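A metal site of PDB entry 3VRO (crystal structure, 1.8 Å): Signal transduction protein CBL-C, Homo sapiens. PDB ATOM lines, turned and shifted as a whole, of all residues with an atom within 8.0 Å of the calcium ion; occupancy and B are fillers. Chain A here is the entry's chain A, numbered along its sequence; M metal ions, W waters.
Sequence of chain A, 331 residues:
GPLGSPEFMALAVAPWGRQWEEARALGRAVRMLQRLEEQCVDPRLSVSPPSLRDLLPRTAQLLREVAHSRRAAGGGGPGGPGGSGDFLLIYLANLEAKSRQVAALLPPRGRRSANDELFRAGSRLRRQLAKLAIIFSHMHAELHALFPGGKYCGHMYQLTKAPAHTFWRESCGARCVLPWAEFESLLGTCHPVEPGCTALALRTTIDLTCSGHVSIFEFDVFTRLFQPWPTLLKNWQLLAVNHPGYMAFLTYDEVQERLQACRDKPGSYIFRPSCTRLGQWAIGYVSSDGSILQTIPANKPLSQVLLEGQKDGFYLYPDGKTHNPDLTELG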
ATOM      1  N   PHE A  87      -3.990 -16.549 -22.731  1.00  0.00           N
ATOM      2  CA  PHE A  87      -3.977 -17.983 -22.390  1.00  0.00           C
ATOM      3  C   PHE A  87      -2.878 -18.681 -23.179  1.00  0.00           C
ATOM      4  O   PHE A  87      -2.088 -19.436 -22.631  1.00  0.00           O
ATOM      5  CB  PHE A  87      -5.328 -18.623 -22.770  1.00  0.00           C
ATOM      6  CG  PHE A  87      -5.307 -20.081 -22.572  1.00  0.00           C
ATOM      7  CD1 PHE A  87      -5.571 -20.622 -21.296  1.00  0.00           C
ATOM      8  CD2 PHE A  87      -4.847 -20.916 -23.597  1.00  0.00           C
ATOM      9  CE1 PHE A  87      -5.458 -22.017 -21.074  1.00  0.00           C
ATOM     10  CE2 PHE A  87      -4.733 -22.331 -23.389  1.00  0.00           C
ATOM     11  CZ  PHE A  87      -4.964 -22.844 -22.073  1.00  0.00           C
ATOM     12  N   ILE A  90       0.944 -17.951 -22.124  1.00  0.00           N
ATOM     13  CA  ILE A  90       1.208 -18.720 -20.929  1.00  0.00           C
ATOM     14  C   ILE A  90       1.313 -20.232 -21.225  1.00  0.00           C
ATOM     15  O   ILE A  90       2.278 -20.912 -20.791  1.00  0.00           O
ATOM     16  CB  ILE A  90       0.128 -18.527 -19.810  1.00  0.00           C
ATOM     17  CG1 ILE A  90      -0.182 -17.041 -19.428  1.00  0.00           C
ATOM     18  CG2 ILE A  90       0.551 -19.320 -18.575  1.00  0.00           C
ATOM     19  CD1 ILE A  90      -1.869 -16.894 -18.956  1.00  0.00           C
ATOM     20  N   TYR A  91       0.330 -20.744 -21.935  1.00  0.00           N
ATOM     21  CA  TYR A  91       0.192 -22.204 -22.142  1.00  0.00           C
ATOM     22  C   TYR A  91       1.416 -22.690 -22.919  1.00  0.00           C
ATOM     23  O   TYR A  91       1.972 -23.738 -22.614  1.00  0.00           O
ATOM     24  CB  TYR A  91      -1.077 -22.487 -22.948  1.00  0.00           C
ATOM     25  CG  TYR A  91      -1.279 -23.933 -23.316  1.00  0.00           C
ATOM     26  CD1 TYR A  91      -1.996 -24.813 -22.485  1.00  0.00           C
ATOM     27  CD2 TYR A  91      -0.749 -24.437 -24.489  1.00  0.00           C
ATOM     28  CE1 TYR A  91      -2.199 -26.148 -22.861  1.00  0.00           C
ATOM     29  CE2 TYR A  91      -0.980 -25.772 -24.879  1.00  0.00           C
ATOM     30  CZ  TYR A  91      -1.689 -26.621 -24.037  1.00  0.00           C
ATOM     31  OH  TYR A  91      -1.853 -27.918 -24.438  1.00  0.00           O
ATOM     32  N   ASN A  94       4.651 -22.707 -20.918  1.00  0.00           N
ATOM     33  CA  ASN A  94       4.646 -23.838 -19.995  1.00  0.00           C
ATOM     34  C   ASN A  94       4.838 -25.135 -20.764  1.00  0.00           C
ATOM     35  O   ASN A  94       5.615 -26.029 -20.310  1.00  0.00           O
ATOM     36  CB  ASN A  94       3.338 -23.873 -19.211  1.00  0.00           C
ATOM     37  CG  ASN A  94       3.336 -24.985 -18.175  1.00  0.00           C
ATOM     38  OD1 ASN A  94       4.209 -25.047 -17.321  1.00  0.00           O
ATOM     39  ND2 ASN A  94       2.363 -25.880 -18.267  1.00  0.00           N
ATOM     40  N   HIS A 138      -3.162 -33.418 -18.922  1.00  0.00           N
ATOM     41  CA  HIS A 138      -3.918 -32.239 -18.473  1.00  0.00           C
ATOM     42  C   HIS A 138      -3.773 -31.084 -19.450  1.00  0.00           C
ATOM     43  O   HIS A 138      -4.777 -30.435 -19.728  1.00  0.00           O
ATOM     44  CB  HIS A 138      -3.411 -31.821 -17.087  1.00  0.00           C
ATOM     45  CG  HIS A 138      -3.732 -32.817 -15.995  1.00  0.00           C
ATOM     46  ND1 HIS A 138      -3.091 -32.824 -14.767  1.00  0.00           N
ATOM     47  CD2 HIS A 138      -4.649 -33.820 -15.943  1.00  0.00           C
ATOM     48  CE1 HIS A 138      -3.615 -33.768 -13.995  1.00  0.00           C
ATOM     49  NE2 HIS A 138      -4.574 -34.377 -14.679  1.00  0.00           N
ATOM     50  N   MET A 139      -2.561 -30.811 -19.963  1.00  0.00           N
ATOM     51  CA  MET A 139      -2.381 -29.757 -20.981  1.00  0.00           C
ATOM     52  C   MET A 139      -3.205 -30.059 -22.212  1.00  0.00           C
ATOM     53  O   MET A 139      -3.773 -29.140 -22.835  1.00  0.00           O
ATOM     54  CB  MET A 139      -0.905 -29.571 -21.371  1.00  0.00           C
ATOM     55  CG  MET A 139      -0.152 -28.995 -20.133  1.00  0.00           C
ATOM     56  SD  MET A 139       1.590 -28.614 -20.594  1.00  0.00           S
ATOM     57  CE  MET A 139       2.225 -30.251 -20.877  1.00  0.00           C
ATOM     58  N   GLU A 142      -6.979 -29.488 -21.333  1.00  0.00           N
ATOM     59  CA  GLU A 142      -7.289 -28.046 -21.185  1.00  0.00           C
ATOM     60  C   GLU A 142      -7.345 -27.354 -22.545  1.00  0.00           C
ATOM     61  O   GLU A 142      -8.228 -26.551 -22.808  1.00  0.00           O
ATOM     62  CB  GLU A 142      -6.185 -27.411 -20.395  1.00  0.00           C
ATOM     63  CG  GLU A 142      -6.451 -25.930 -20.111  1.00  0.00           C
ATOM     64  CD  GLU A 142      -5.256 -25.327 -19.297  1.00  0.00           C
ATOM     65  OE1 GLU A 142      -4.132 -25.343 -19.825  1.00  0.00           O
ATOM     66  OE2 GLU A 142      -5.466 -24.846 -18.142  1.00  0.00           O
ATOM     67  N   VAL A 177      -8.577 -17.515 -17.869  1.00  0.00           N
ATOM     68  CA  VAL A 177      -7.336 -17.863 -17.155  1.00  0.00           C
ATOM     69  C   VAL A 177      -6.864 -16.692 -16.308  1.00  0.00           C
ATOM     70  O   VAL A 177      -7.041 -15.517 -16.729  1.00  0.00           O
ATOM     71  CB  VAL A 177      -6.186 -18.358 -18.109  1.00  0.00           C
ATOM     72  CG1 VAL A 177      -5.733 -17.246 -19.075  1.00  0.00           C
ATOM     73  CG2 VAL A 177      -5.014 -18.862 -17.324  1.00  0.00           C
ATOM     74  N   LEU A 178      -6.335 -16.993 -15.117  1.00  0.00           N
ATOM     75  CA  LEU A 178      -5.825 -15.975 -14.161  1.00  0.00           C
ATOM     76  C   LEU A 178      -4.518 -16.467 -13.611  1.00  0.00           C
ATOM     77  O   LEU A 178      -4.365 -17.681 -13.390  1.00  0.00           O
ATOM     78  CB  LEU A 178      -6.827 -15.824 -12.934  1.00  0.00           C
ATOM     79  CG  LEU A 178      -7.903 -14.779 -13.255  1.00  0.00           C
ATOM     80  CD1 LEU A 178      -9.057 -15.446 -14.028  1.00  0.00           C
ATOM     81  CD2 LEU A 178      -8.383 -14.042 -11.994  1.00  0.00           C
ATOM     82  N   ARG A 203      -2.861 -24.624  -4.252  1.00  0.00           N
ATOM     83  CA  ARG A 203      -2.319 -24.309  -5.585  1.00  0.00           C
ATOM     84  C   ARG A 203      -1.917 -25.556  -6.340  1.00  0.00           C
ATOM     85  O   ARG A 203      -2.281 -25.750  -7.540  1.00  0.00           O
ATOM     86  CB  ARG A 203      -1.156 -23.322  -5.425  1.00  0.00           C
ATOM     87  CG  ARG A 203      -0.533 -23.010  -6.803  1.00  0.00           C
ATOM     88  CD  ARG A 203       0.576 -21.962  -6.566  1.00  0.00           C
ATOM     89  NE  ARG A 203       1.377 -21.823  -7.806  1.00  0.00           N
ATOM     90  CZ  ARG A 203       2.055 -20.701  -8.132  1.00  0.00           C
ATOM     91  NH1 ARG A 203       1.971 -19.634  -7.364  1.00  0.00           N
ATOM     92  NH2 ARG A 203       2.794 -20.688  -9.251  1.00  0.00           N
ATOM     93  N   ILE A 206      -5.070 -27.459  -7.534  1.00  0.00           N
ATOM     94  CA  ILE A 206      -5.839 -26.808  -8.605  1.00  0.00           C
ATOM     95  C   ILE A 206      -5.048 -26.785  -9.900  1.00  0.00           C
ATOM     96  O   ILE A 206      -5.620 -26.989 -10.986  1.00  0.00           O
ATOM     97  CB  ILE A 206      -6.275 -25.415  -8.210  1.00  0.00           C
ATOM     98  CG1 ILE A 206      -7.327 -25.559  -7.076  1.00  0.00           C
ATOM     99  CG2 ILE A 206      -6.783 -24.513  -9.396  1.00  0.00           C
ATOM    100  CD1 ILE A 206      -7.745 -24.155  -6.507  1.00  0.00           C
ATOM    101  N   ASP A 207      -3.752 -26.583  -9.798  1.00  0.00           N
ATOM    102  CA  ASP A 207      -2.978 -26.289 -11.045  1.00  0.00           C
ATOM    103  C   ASP A 207      -2.575 -27.609 -11.726  1.00  0.00           C
ATOM    104  O   ASP A 207      -1.441 -28.135 -11.571  1.00  0.00           O
ATOM    105  CB  ASP A 207      -1.726 -25.457 -10.653  1.00  0.00           C
ATOM    106  CG  ASP A 207      -0.924 -24.951 -11.824  1.00  0.00           C
ATOM    107  OD1 ASP A 207      -1.331 -25.178 -12.991  1.00  0.00           O
ATOM    108  OD2 ASP A 207       0.153 -24.350 -11.544  1.00  0.00           O
ATOM    109  N   LEU A 208      -3.494 -28.114 -12.542  1.00  0.00           N
ATOM    110  CA  LEU A 208      -3.336 -29.402 -13.246  1.00  0.00           C
ATOM    111  C   LEU A 208      -2.175 -29.391 -14.236  1.00  0.00           C
ATOM    112  O   LEU A 208      -1.539 -30.427 -14.449  1.00  0.00           O
ATOM    113  CB  LEU A 208      -4.589 -29.638 -14.117  1.00  0.00           C
ATOM    114  CG  LEU A 208      -5.873 -29.855 -13.289  1.00  0.00           C
ATOM    115  CD1 LEU A 208      -7.036 -30.160 -14.240  1.00  0.00           C
ATOM    116  CD2 LEU A 208      -5.725 -30.934 -12.137  1.00  0.00           C
ATOM    117  N   THR A 209      -1.963 -28.242 -14.859  1.00  0.00           N
ATOM    118  CA  THR A 209      -0.901 -28.128 -15.888  1.00  0.00           C
ATOM    119  C   THR A 209       0.441 -27.673 -15.283  1.00  0.00           C
ATOM    120  O   THR A 209       1.418 -27.591 -16.006  1.00  0.00           O
ATOM    121  CB  THR A 209      -1.369 -27.180 -17.004  1.00  0.00           C
ATOM    122  OG1 THR A 209      -1.570 -25.825 -16.514  1.00  0.00           O
ATOM    123  CG2 THR A 209      -2.712 -27.730 -17.610  1.00  0.00           C
ATOM    124  N   CYS A 210       0.443 -27.377 -13.979  1.00  0.00           N
ATOM    125  CA  CYS A 210       1.642 -26.920 -13.236  1.00  0.00           C
ATOM    126  C   CYS A 210       2.195 -25.712 -13.922  1.00  0.00           C
ATOM    127  O   CYS A 210       3.434 -25.545 -14.025  1.00  0.00           O
ATOM    128  CB  CYS A 210       2.692 -28.026 -13.153  1.00  0.00           C
ATOM    129  SG  CYS A 210       2.173 -29.398 -12.194  1.00  0.00           S
ATOM    130  N   SER A 211       1.283 -24.851 -14.400  1.00  0.00           N
ATOM    131  CA  SER A 211       1.628 -23.637 -15.165  1.00  0.00           C
ATOM    132  C   SER A 211       1.748 -22.378 -14.300  1.00  0.00           C
ATOM    133  O   SER A 211       2.155 -21.317 -14.822  1.00  0.00           O
ATOM    134  CB  SER A 211       0.535 -23.356 -16.249  1.00  0.00           C
ATOM    135  OG  SER A 211      -0.645 -22.872 -15.646  1.00  0.00           O
ATOM    136  N   GLY A 212       1.312 -22.443 -13.044  1.00  0.00           N
ATOM    137  CA  GLY A 212       1.208 -21.224 -12.230  1.00  0.00           C
ATOM    138  C   GLY A 212      -0.014 -20.364 -12.452  1.00  0.00           C
ATOM    139  O   GLY A 212      -0.170 -19.315 -11.857  1.00  0.00           O
ATOM    140  N   HIS A 213      -0.881 -20.780 -13.388  1.00  0.00           N
ATOM    141  CA  HIS A 213      -2.072 -19.994 -13.703  1.00  0.00           C
ATOM    142  C   HIS A 213      -3.244 -20.962 -13.609  1.00  0.00           C
ATOM    143  O   HIS A 213      -3.061 -22.160 -13.748  1.00  0.00           O
ATOM    144  CB  HIS A 213      -1.989 -19.487 -15.172  1.00  0.00           C
ATOM    145  CG  HIS A 213      -1.008 -18.396 -15.348  1.00  0.00           C
ATOM    146  ND1 HIS A 213       0.352 -18.620 -15.253  1.00  0.00           N
ATOM    147  CD2 HIS A 213      -1.162 -17.070 -15.579  1.00  0.00           C
ATOM    148  CE1 HIS A 213       0.994 -17.463 -15.430  1.00  0.00           C
ATOM    149  NE2 HIS A 213       0.095 -16.522 -15.612  1.00  0.00           N
ATOM    150  N   VAL A 214      -4.424 -20.457 -13.310  1.00  0.00           N
ATOM    151  CA  VAL A 214      -5.608 -21.291 -13.143  1.00  0.00           C
ATOM    152  C   VAL A 214      -6.520 -20.988 -14.336  1.00  0.00           C
ATOM    153  O   VAL A 214      -6.965 -19.866 -14.442  1.00  0.00           O
ATOM    154  CB  VAL A 214      -6.307 -20.927 -11.808  1.00  0.00           C
ATOM    155  CG1 VAL A 214      -7.634 -21.747 -11.582  1.00  0.00           C
ATOM    156  CG2 VAL A 214      -5.263 -21.230 -10.649  1.00  0.00           C
ATOM    157  N   SER A 215      -6.807 -21.969 -15.204  1.00  0.00           N
ATOM    158  CA  SER A 215      -7.818 -21.744 -16.245  1.00  0.00           C
ATOM    159  C   SER A 215      -9.197 -22.097 -15.746  1.00  0.00           C
ATOM    160  O   SER A 215      -9.398 -22.723 -14.689  1.00  0.00           O
ATOM    161  CB  SER A 215      -7.580 -22.599 -17.488  1.00  0.00           C
ATOM    162  OG  SER A 215      -7.714 -23.952 -17.113  1.00  0.00           O
ATOM    163  N   GLU A 218      -9.414 -25.801 -15.277  1.00  0.00           N
ATOM    164  CA  GLU A 218      -8.900 -26.320 -14.018  1.00  0.00           C
ATOM    165  C   GLU A 218      -9.866 -26.020 -12.924  1.00  0.00           C
ATOM    166  O   GLU A 218     -10.022 -26.850 -12.009  1.00  0.00           O
ATOM    167  CB  GLU A 218      -7.557 -25.668 -13.696  1.00  0.00           C
ATOM    168  CG  GLU A 218      -6.495 -26.323 -14.622  1.00  0.00           C
ATOM    169  CD  GLU A 218      -5.239 -25.452 -14.603  1.00  0.00           C
ATOM    170  OE1 GLU A 218      -5.358 -24.187 -14.565  1.00  0.00           O
ATOM    171  OE2 GLU A 218      -4.147 -26.025 -14.616  1.00  0.00           O
HETATM  172 CA    CA M   1      -2.531 -24.313 -14.807  1.00  0.00          CA
HETATM  173  O   HOH W   1      -3.910 -23.250 -16.639  1.00  0.00           O
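The side-chain carboxylate of Asp 207 sits close to the backbone NH of Cys 210, at 3.0 Å.
OD2 of Asp 207 sits at hydrogen-bond distance from N of Gly 212 (2.7 Å).
The side-chain carboxylate (OE2) of Glu 218 lies close to the backbone NH (N) of Leu 208, 3.0 Å away.
The backbone NH (N) of Glu 218 sits at hydrogen-bond distance from the side-chain hydroxyl (OG) of Ser 215 (3.1 Å).
The side-chain amide nitrogen (ND2) of Asn 94 is in hydrogen-bond range of the backbone carbonyl oxygen (O) of Thr 209 (3.0 Å).
Five residues have an atom within 4 Å of the calcium ion: Asp 207, Thr 209, Ser 211, His 213 and Glu 218.
The nearest printed residue that does not touch the calcium ion is Cys 210 (4.3 Å).
The calcium ion is bound by OD1 of Asp 207 (2.3 Å).
The calcium ion is bound by OE2 of Glu 218, at 2.4 Å.
O of His 213 binds the calcium ion, at 2.5 Å.
OG1 of Thr 209 binds the calcium ion, at 2.5 Å.
The calcium ion is bound by OG of Ser 211, at 2.5 Å.
The calcium ion is bound by water W1.
The calcium ion is bound by OE1 of Glu 218 (2.8 Å).
The calcium ion has seven donor atoms within binding distance.
Water W1 bridges the side-chain carboxylate of Glu 142 and the backbone NH of Ser 215.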
